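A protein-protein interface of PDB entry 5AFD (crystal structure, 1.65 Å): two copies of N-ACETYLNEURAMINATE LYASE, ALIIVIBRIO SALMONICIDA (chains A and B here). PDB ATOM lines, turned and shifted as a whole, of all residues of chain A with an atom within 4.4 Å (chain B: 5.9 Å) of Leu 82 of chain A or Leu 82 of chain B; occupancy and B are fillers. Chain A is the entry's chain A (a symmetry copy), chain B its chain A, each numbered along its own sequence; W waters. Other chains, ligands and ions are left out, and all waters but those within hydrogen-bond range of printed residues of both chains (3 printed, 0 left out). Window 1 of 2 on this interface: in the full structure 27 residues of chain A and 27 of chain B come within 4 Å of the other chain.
The backbone carbonyl oxygen (O) of Ser 83 of chain B is in hydrogen-bond range of the side-chain hydroxyl (OG1) of Thr 87 of chain B (3.2 Å).
The backbone carbonyl oxygen of Ile 51 of chain B lies within hydrogen-bond range of the backbone NH of Ser 83 of chain A (3.2 Å).
O of His 52 of chain B lies within hydrogen-bond range of OG of Ser 83 of chain A, 2.8 Å away.
The backbone NH of Ser 83 of chain B sits at hydrogen-bond distance from the backbone carbonyl oxygen of Ile 51 of chain A, at 3.2 Å.
OG of Ser 83 of chain B is in hydrogen-bond range of O of His 52 of chain A, 2.8 Å away.
The backbone carbonyl oxygen (O) of Cys 108 of chain B lies close to the side-chain sulfur (SG) of Cys 108 of chain A, at 3.7 Å.
Ile 51 of chain A touches Leu 82 of chain B, and with the chains exchanged Leu 82 of chain A touches Ile 51 of chain B.
Ile 51 of chain A touches Ser 83 of chain B, and with the chains exchanged Ser 83 of chain A touches Ile 51 of chain B.
Ile 51 of chain A touches Phe 109 of chain B, and with the chains exchanged Phe 109 of chain A touches Ile 51 of chain B.
Cys 108 of chain A touches its own counterpart, Cys 108 of chain B.
Positions printed for both chains: 51, 52, 81, 82, 83, 84, 108 and 109.
Of the 14 printed residues of chain B, 7 touch a printed residue of chain A.
Of the 8 printed residues of chain A, 7 touch a printed residue of chain B.
Printed residues of chain A that touch a printed residue of chain B: Ile 51, His 52, Leu 82, Ser 83, Ile 84, Cys 108 and Phe 109.
Hydrophobic or aromatic side chains of chain A within 4 Å of the printed part of chain B: Ile 51, His 52, Leu 82, Ile 84 and Phe 109.
Among the printed residues, 15 pairs touch across the chains.
Among the printed residues, no Asp or Glu carboxylate lies within 4 Å of a Lys or Arg side-chain nitrogen of the other chain.
Water W2 lies within hydrogen-bond range of O of Leu 273 of chain B (2.7 Å), O of Leu 82 of chain A (2.8 Å) and N of Ile 84 of chain A (2.8 Å).
Water W3 bridges NE2 of His 52 of chain B (2.8 Å) and O of Leu 82 of chain A (3.1 Å).
Water W1 lies within hydrogen-bond range of NE2 of His 52 of chain A and O of Leu 82 of chain B.
Of the printed residues of chain B, Leu 82 of chain A touches Ile 51 (3.4 Å), His 52 (3.5 Å) and Leu 82 (3.6 Å).
Leu 82 of chain B touches three residues of chain A.
Of the printed residues of chain B, His 52 of chain A touches Leu 82 and Ser 83.
Printed residues of chain A within 4 Å of Leu 273 of chain B: Ile 84.
Of the printed residues of chain B, Ile 84 of chain A touches Leu 273.
Printed residues of chain A within 4 Å of Ile 51 of chain B: Leu 82, Ser 83 and Phe 109.
Of the printed residues of chain A, Ser 83 of chain B touches Ile 51 and His 52.
Tyr 121 of chain B touches none of the printed residues of chain A.
The nearest printed residue of chain B that does not touch Ser 83 of chain A is Leu 273 of chain B (5.7 Å).
Among the printed residues, merely in contact across the chains: Ile 51 of chain A with Leu 82 of chain B (3.4 Å), Ile 51 of chain A with Phe 109 of chain B (3.6 Å), His 52 of chain A with Leu 82 of chain B (3.5 Å), Leu 82 of chain A with Ile 51 of chain B (3.4 Å), Leu 82 of chain A with His 52 of chain B (3.5 Å), Leu 82 of chain A with Leu 82 of chain B (3.6 Å), Ile 84 of chain A with Leu 273 of chain B (3.8 Å), Cys 108 of chain A with Phe 109 of chain B (3.9 Å), Phe 109 of chain A with Ile 51 of chain B (3.6 Å) and Phe 109 of chain A with Cys 108 of chain B (3.9 Å).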
ATOM      1  N   ILE A  51     -17.406 -14.605   4.797  1.00  0.00           N
ATOM      2  CA  ILE A  51     -18.140 -13.828   5.790  1.00  0.00           C
ATOM      3  C   ILE A  51     -18.287 -14.585   7.097  1.00  0.00           C
ATOM      4  O   ILE A  51     -18.674 -13.978   8.073  1.00  0.00           O
ATOM      5  CB  ILE A  51     -19.595 -13.441   5.248  1.00  0.00           C
ATOM      6  CG1 ILE A  51     -20.311 -14.765   4.865  1.00  0.00           C
ATOM      7  CG2 ILE A  51     -19.440 -12.311   4.206  1.00  0.00           C
ATOM      8  CD1 ILE A  51     -21.812 -14.600   4.733  1.00  0.00           C
ATOM      9  N   HIS A  52     -17.989 -15.892   7.154  1.00  0.00           N
ATOM     10  CA  HIS A  52     -17.986 -16.604   8.448  1.00  0.00           C
ATOM     11  C   HIS A  52     -16.656 -16.454   9.213  1.00  0.00           C
ATOM     12  O   HIS A  52     -16.555 -16.963  10.359  1.00  0.00           O
ATOM     13  CB  HIS A  52     -18.301 -18.075   8.274  1.00  0.00           C
ATOM     14  CG  HIS A  52     -19.724 -18.272   7.818  1.00  0.00           C
ATOM     15  ND1 HIS A  52     -20.218 -19.500   7.381  1.00  0.00           N
ATOM     16  CD2 HIS A  52     -20.734 -17.358   7.681  1.00  0.00           C
ATOM     17  CE1 HIS A  52     -21.519 -19.337   7.065  1.00  0.00           C
ATOM     18  NE2 HIS A  52     -21.860 -18.061   7.268  1.00  0.00           N
ATOM     19  N   ALA A  81     -17.657  -7.353   3.432  1.00  0.00           N
ATOM     20  CA  ALA A  81     -18.092  -7.593   4.831  1.00  0.00           C
ATOM     21  C   ALA A  81     -19.237  -6.584   5.046  1.00  0.00           C
ATOM     22  O   ALA A  81     -19.370  -5.591   4.308  1.00  0.00           O
ATOM     23  CB  ALA A  81     -16.938  -7.461   5.823  1.00  0.00           C
ATOM     24  N   LEU A  82     -20.071  -6.812   6.067  1.00  0.00           N
ATOM     25  CA  LEU A  82     -21.102  -5.816   6.300  1.00  0.00           C
ATOM     26  C   LEU A  82     -20.510  -4.444   6.766  1.00  0.00           C
ATOM     27  O   LEU A  82     -21.112  -3.361   6.538  1.00  0.00           O
ATOM     28  CB  LEU A  82     -22.161  -6.338   7.285  1.00  0.00           C
ATOM     29  CG  LEU A  82     -23.055  -7.489   6.821  1.00  0.00           C
ATOM     30  CD1 LEU A  82     -24.106  -7.861   7.853  1.00  0.00           C
ATOM     31  CD2 LEU A  82     -23.716  -7.007   5.551  1.00  0.00           C
ATOM     32  N   SER A  83     -19.380  -4.457   7.491  1.00  0.00           N
ATOM     33  CA  SER A  83     -18.766  -3.192   8.008  1.00  0.00           C
ATOM     34  C   SER A  83     -17.729  -2.720   6.960  1.00  0.00           C
ATOM     35  O   SER A  83     -16.872  -3.470   6.536  1.00  0.00           O
ATOM     36  CB  SER A  83     -17.963  -3.518   9.297  1.00  0.00           C
ATOM     37  OG  SER A  83     -17.234  -2.302   9.611  1.00  0.00           O
ATOM     38  N   ILE A  84     -17.881  -1.483   6.506  1.00  0.00           N
ATOM     39  CA  ILE A  84     -16.978  -0.870   5.535  1.00  0.00           C
ATOM     40  C   ILE A  84     -15.570  -0.802   6.176  1.00  0.00           C
ATOM     41  O   ILE A  84     -14.532  -0.795   5.491  1.00  0.00           O
ATOM     42  CB  ILE A  84     -17.525   0.551   5.127  1.00  0.00           C
ATOM     43  CG1 ILE A  84     -16.704   1.173   3.948  1.00  0.00           C
ATOM     44  CG2 ILE A  84     -17.714   1.480   6.344  1.00  0.00           C
ATOM     45  CD1 ILE A  84     -16.720   0.339   2.684  1.00  0.00           C
ATOM     46  N   CYS A 108     -26.012  -7.357   2.252  1.00  0.00           N
ATOM     47  CA  CYS A 108     -27.284  -8.012   2.278  1.00  0.00           C
ATOM     48  C   CYS A 108     -28.219  -7.485   3.345  1.00  0.00           C
ATOM     49  O   CYS A 108     -29.338  -7.997   3.441  1.00  0.00           O
ATOM     50  CB  CYS A 108     -27.098  -9.561   2.447  1.00  0.00           C
ATOM     51  SG  CYS A 108     -26.237 -10.094   3.904  1.00  0.00           S
ATOM     52  N   PHE A 109     -27.800  -6.500   4.151  1.00  0.00           N
ATOM     53  CA  PHE A 109     -28.696  -6.090   5.255  1.00  0.00           C
ATOM     54  C   PHE A 109     -29.312  -4.742   4.832  1.00  0.00           C
ATOM     55  O   PHE A 109     -30.425  -4.727   4.415  1.00  0.00           O
ATOM     56  CB  PHE A 109     -28.030  -6.032   6.631  1.00  0.00           C
ATOM     57  CG  PHE A 109     -29.072  -5.954   7.705  1.00  0.00           C
ATOM     58  CD1 PHE A 109     -29.844  -7.073   8.003  1.00  0.00           C
ATOM     59  CD2 PHE A 109     -29.348  -4.758   8.377  1.00  0.00           C
ATOM     60  CE1 PHE A 109     -30.854  -7.055   8.971  1.00  0.00           C
ATOM     61  CE2 PHE A 109     -30.413  -4.713   9.318  1.00  0.00           C
ATOM     62  CZ  PHE A 109     -31.164  -5.871   9.619  1.00  0.00           C
ATOM     63  N   ILE B  51     -23.660  -3.439  12.659  1.00  0.00           N
ATOM     64  CA  ILE B  51     -22.982  -4.223  11.633  1.00  0.00           C
ATOM     65  C   ILE B  51     -22.096  -3.357  10.758  1.00  0.00           C
ATOM     66  O   ILE B  51     -21.308  -3.904  10.017  1.00  0.00           O
ATOM     67  CB  ILE B  51     -24.042  -4.984  10.706  1.00  0.00           C
ATOM     68  CG1 ILE B  51     -24.993  -3.908  10.115  1.00  0.00           C
ATOM     69  CG2 ILE B  51     -24.615  -6.177  11.504  1.00  0.00           C
ATOM     70  CD1 ILE B  51     -25.770  -4.412   8.916  1.00  0.00           C
ATOM     71  N   HIS B  52     -22.193  -2.020  10.818  1.00  0.00           N
ATOM     72  CA  HIS B  52     -21.238  -1.165  10.084  1.00  0.00           C
ATOM     73  C   HIS B  52     -19.929  -0.923  10.861  1.00  0.00           C
ATOM     74  O   HIS B  52     -19.010  -0.263  10.311  1.00  0.00           O
ATOM     75  CB  HIS B  52     -21.855   0.167   9.714  1.00  0.00           C
ATOM     76  CG  HIS B  52     -22.953  -0.011   8.697  1.00  0.00           C
ATOM     77  ND1 HIS B  52     -23.826   1.014   8.335  1.00  0.00           N
ATOM     78  CD2 HIS B  52     -23.343  -1.133   8.016  1.00  0.00           C
ATOM     79  CE1 HIS B  52     -24.669   0.532   7.399  1.00  0.00           C
ATOM     80  NE2 HIS B  52     -24.375  -0.751   7.168  1.00  0.00           N
ATOM     81  N   GLY B  80     -24.831  -9.637  17.212  1.00  0.00           N
ATOM     82  CA  GLY B  80     -24.831 -10.431  15.951  1.00  0.00           C
ATOM     83  C   GLY B  80     -23.914  -9.804  14.871  1.00  0.00           C
ATOM     84  O   GLY B  80     -23.808  -8.592  14.731  1.00  0.00           O
ATOM     85  N   ALA B  81     -23.365 -10.684  14.050  1.00  0.00           N
ATOM     86  CA  ALA B  81     -22.421 -10.368  12.948  1.00  0.00           C
ATOM     87  C   ALA B  81     -22.552 -11.567  11.987  1.00  0.00           C
ATOM     88  O   ALA B  81     -23.030 -12.651  12.369  1.00  0.00           O
ATOM     89  CB  ALA B  81     -21.004 -10.118  13.459  1.00  0.00           C
ATOM     90  N   LEU B  82     -22.115 -11.398  10.734  1.00  0.00           N
ATOM     91  CA  LEU B  82     -22.181 -12.557   9.862  1.00  0.00           C
ATOM     92  C   LEU B  82     -21.205 -13.695  10.311  1.00  0.00           C
ATOM     93  O   LEU B  82     -21.446 -14.904  10.047  1.00  0.00           O
ATOM     94  CB  LEU B  82     -21.944 -12.157   8.395  1.00  0.00           C
ATOM     95  CG  LEU B  82     -23.011 -11.298   7.714  1.00  0.00           C
ATOM     96  CD1 LEU B  82     -22.698 -11.035   6.251  1.00  0.00           C
ATOM     97  CD2 LEU B  82     -24.302 -12.071   7.844  1.00  0.00           C
ATOM     98  N   SER B  83     -20.059 -13.344  10.916  1.00  0.00           N
ATOM     99  CA  SER B  83     -19.053 -14.369  11.345  1.00  0.00           C
ATOM    100  C   SER B  83     -19.365 -14.733  12.817  1.00  0.00           C
ATOM    101  O   SER B  83     -19.492 -13.874  13.667  1.00  0.00           O
ATOM    102  CB  SER B  83     -17.646 -13.714  11.348  1.00  0.00           C
ATOM    103  OG  SER B  83     -16.770 -14.691  11.971  1.00  0.00           O
ATOM    104  N   ILE B  84     -19.555 -16.020  13.070  1.00  0.00           N
ATOM    105  CA  ILE B  84     -19.831 -16.541  14.407  1.00  0.00           C
ATOM    106  C   ILE B  84     -18.610 -16.217  15.303  1.00  0.00           C
ATOM    107  O   ILE B  84     -18.711 -16.085  16.535  1.00  0.00           O
ATOM    108  CB  ILE B  84     -20.127 -18.087  14.323  1.00  0.00           C
ATOM    109  CG1 ILE B  84     -20.618 -18.659  15.695  1.00  0.00           C
ATOM    110  CG2 ILE B  84     -18.969 -18.872  13.672  1.00  0.00           C
ATOM    111  CD1 ILE B  84     -21.891 -18.017  16.206  1.00  0.00           C
ATOM    112  N   THR B  87     -19.170 -12.706  16.345  1.00  0.00           N
ATOM    113  CA  THR B  87     -20.328 -12.742  17.271  1.00  0.00           C
ATOM    114  C   THR B  87     -19.965 -13.270  18.666  1.00  0.00           C
ATOM    115  O   THR B  87     -20.299 -12.680  19.690  1.00  0.00           O
ATOM    116  CB  THR B  87     -21.511 -13.578  16.711  1.00  0.00           C
ATOM    117  OG1 THR B  87     -21.926 -12.959  15.511  1.00  0.00           O
ATOM    118  CG2 THR B  87     -22.660 -13.608  17.708  1.00  0.00           C
ATOM    119  N   PRO B 107     -29.106 -14.052  10.672  1.00  0.00           N
ATOM    120  CA  PRO B 107     -28.111 -13.762   9.661  1.00  0.00           C
ATOM    121  C   PRO B 107     -28.733 -13.651   8.225  1.00  0.00           C
ATOM    122  O   PRO B 107     -29.577 -14.490   7.875  1.00  0.00           O
ATOM    123  CB  PRO B 107     -27.117 -14.979   9.753  1.00  0.00           C
ATOM    124  CG  PRO B 107     -27.529 -15.808  10.865  1.00  0.00           C
ATOM    125  CD  PRO B 107     -28.766 -15.215  11.520  1.00  0.00           C
ATOM    126  N   CYS B 108     -28.278 -12.653   7.478  1.00  0.00           N
ATOM    127  CA  CYS B 108     -28.992 -12.293   6.292  1.00  0.00           C
ATOM    128  C   CYS B 108     -28.400 -12.871   5.025  1.00  0.00           C
ATOM    129  O   CYS B 108     -28.952 -12.607   3.952  1.00  0.00           O
ATOM    130  CB  CYS B 108     -29.098 -10.733   6.169  1.00  0.00           C
ATOM    131  SG  CYS B 108     -27.564  -9.843   6.112  1.00  0.00           S
ATOM    132  N   PHE B 109     -27.298 -13.630   5.107  1.00  0.00           N
ATOM    133  CA  PHE B 109     -26.681 -14.082   3.840  1.00  0.00           C
ATOM    134  C   PHE B 109     -27.037 -15.574   3.694  1.00  0.00           C
ATOM    135  O   PHE B 109     -27.911 -15.884   2.950  1.00  0.00           O
ATOM    136  CB  PHE B 109     -25.178 -13.817   3.731  1.00  0.00           C
ATOM    137  CG  PHE B 109     -24.727 -13.983   2.312  1.00  0.00           C
ATOM    138  CD1 PHE B 109     -25.076 -13.031   1.359  1.00  0.00           C
ATOM    139  CD2 PHE B 109     -24.019 -15.114   1.892  1.00  0.00           C
ATOM    140  CE1 PHE B 109     -24.714 -13.145   0.012  1.00  0.00           C
ATOM    141  CE2 PHE B 109     -23.700 -15.270   0.515  1.00  0.00           C
ATOM    142  CZ  PHE B 109     -24.045 -14.275  -0.426  1.00  0.00           C
ATOM    143  N   TYR B 121     -28.240 -21.980  16.260  1.00  0.00           N
ATOM    144  CA  TYR B 121     -27.409 -20.757  16.133  1.00  0.00           C
ATOM    145  C   TYR B 121     -27.586 -19.842  17.392  1.00  0.00           C
ATOM    146  O   TYR B 121     -26.593 -19.433  18.036  1.00  0.00           O
ATOM    147  CB  TYR B 121     -27.951 -20.013  14.881  1.00  0.00           C
ATOM    148  CG  TYR B 121     -27.329 -18.630  14.641  1.00  0.00           C
ATOM    149  CD1 TYR B 121     -25.973 -18.556  14.219  1.00  0.00           C
ATOM    150  CD2 TYR B 121     -28.015 -17.438  14.879  1.00  0.00           C
ATOM    151  CE1 TYR B 121     -25.338 -17.314  13.967  1.00  0.00           C
ATOM    152  CE2 TYR B 121     -27.370 -16.178  14.649  1.00  0.00           C
ATOM    153  CZ  TYR B 121     -26.036 -16.137  14.177  1.00  0.00           C
ATOM    154  OH  TYR B 121     -25.379 -14.914  13.948  1.00  0.00           O
ATOM    155  N   LEU B 273     -21.392   4.130   4.731  1.00  0.00           N
ATOM    156  CA  LEU B 273     -21.579   3.224   3.551  1.00  0.00           C
ATOM    157  C   LEU B 273     -21.816   1.789   3.996  1.00  0.00           C
ATOM    158  O   LEU B 273     -21.222   1.316   4.957  1.00  0.00           O
ATOM    159  CB  LEU B 273     -20.334   3.322   2.612  1.00  0.00           C
ATOM    160  CG  LEU B 273     -20.250   4.657   1.853  1.00  0.00           C
ATOM    161  CD1 LEU B 273     -18.957   4.709   1.048  1.00  0.00           C
ATOM    162  CD2 LEU B 273     -21.445   4.735   0.878  1.00  0.00           C
ATOM    163  N   PRO B 274     -22.775   1.088   3.375  1.00  0.00           N
ATOM    164  CA  PRO B 274     -23.504   1.410   2.117  1.00  0.00           C
ATOM    165  C   PRO B 274     -24.692   2.367   2.220  1.00  0.00           C
ATOM    166  O   PRO B 274     -25.292   2.747   1.157  1.00  0.00           O
ATOM    167  CB  PRO B 274     -23.971   0.020   1.618  1.00  0.00           C
ATOM    168  CG  PRO B 274     -24.232  -0.668   2.963  1.00  0.00           C
ATOM    169  CD  PRO B 274     -22.999  -0.326   3.794  1.00  0.00           C
HETATM  170  O   HOH W   1     -23.545 -16.034   8.065  1.00  0.00           O
HETATM  171  O   HOH W   2     -20.580  -0.638   6.634  1.00  0.00           O
HETATM  172  O   HOH W   3     -24.037  -2.978   5.585  1.00  0.00           O
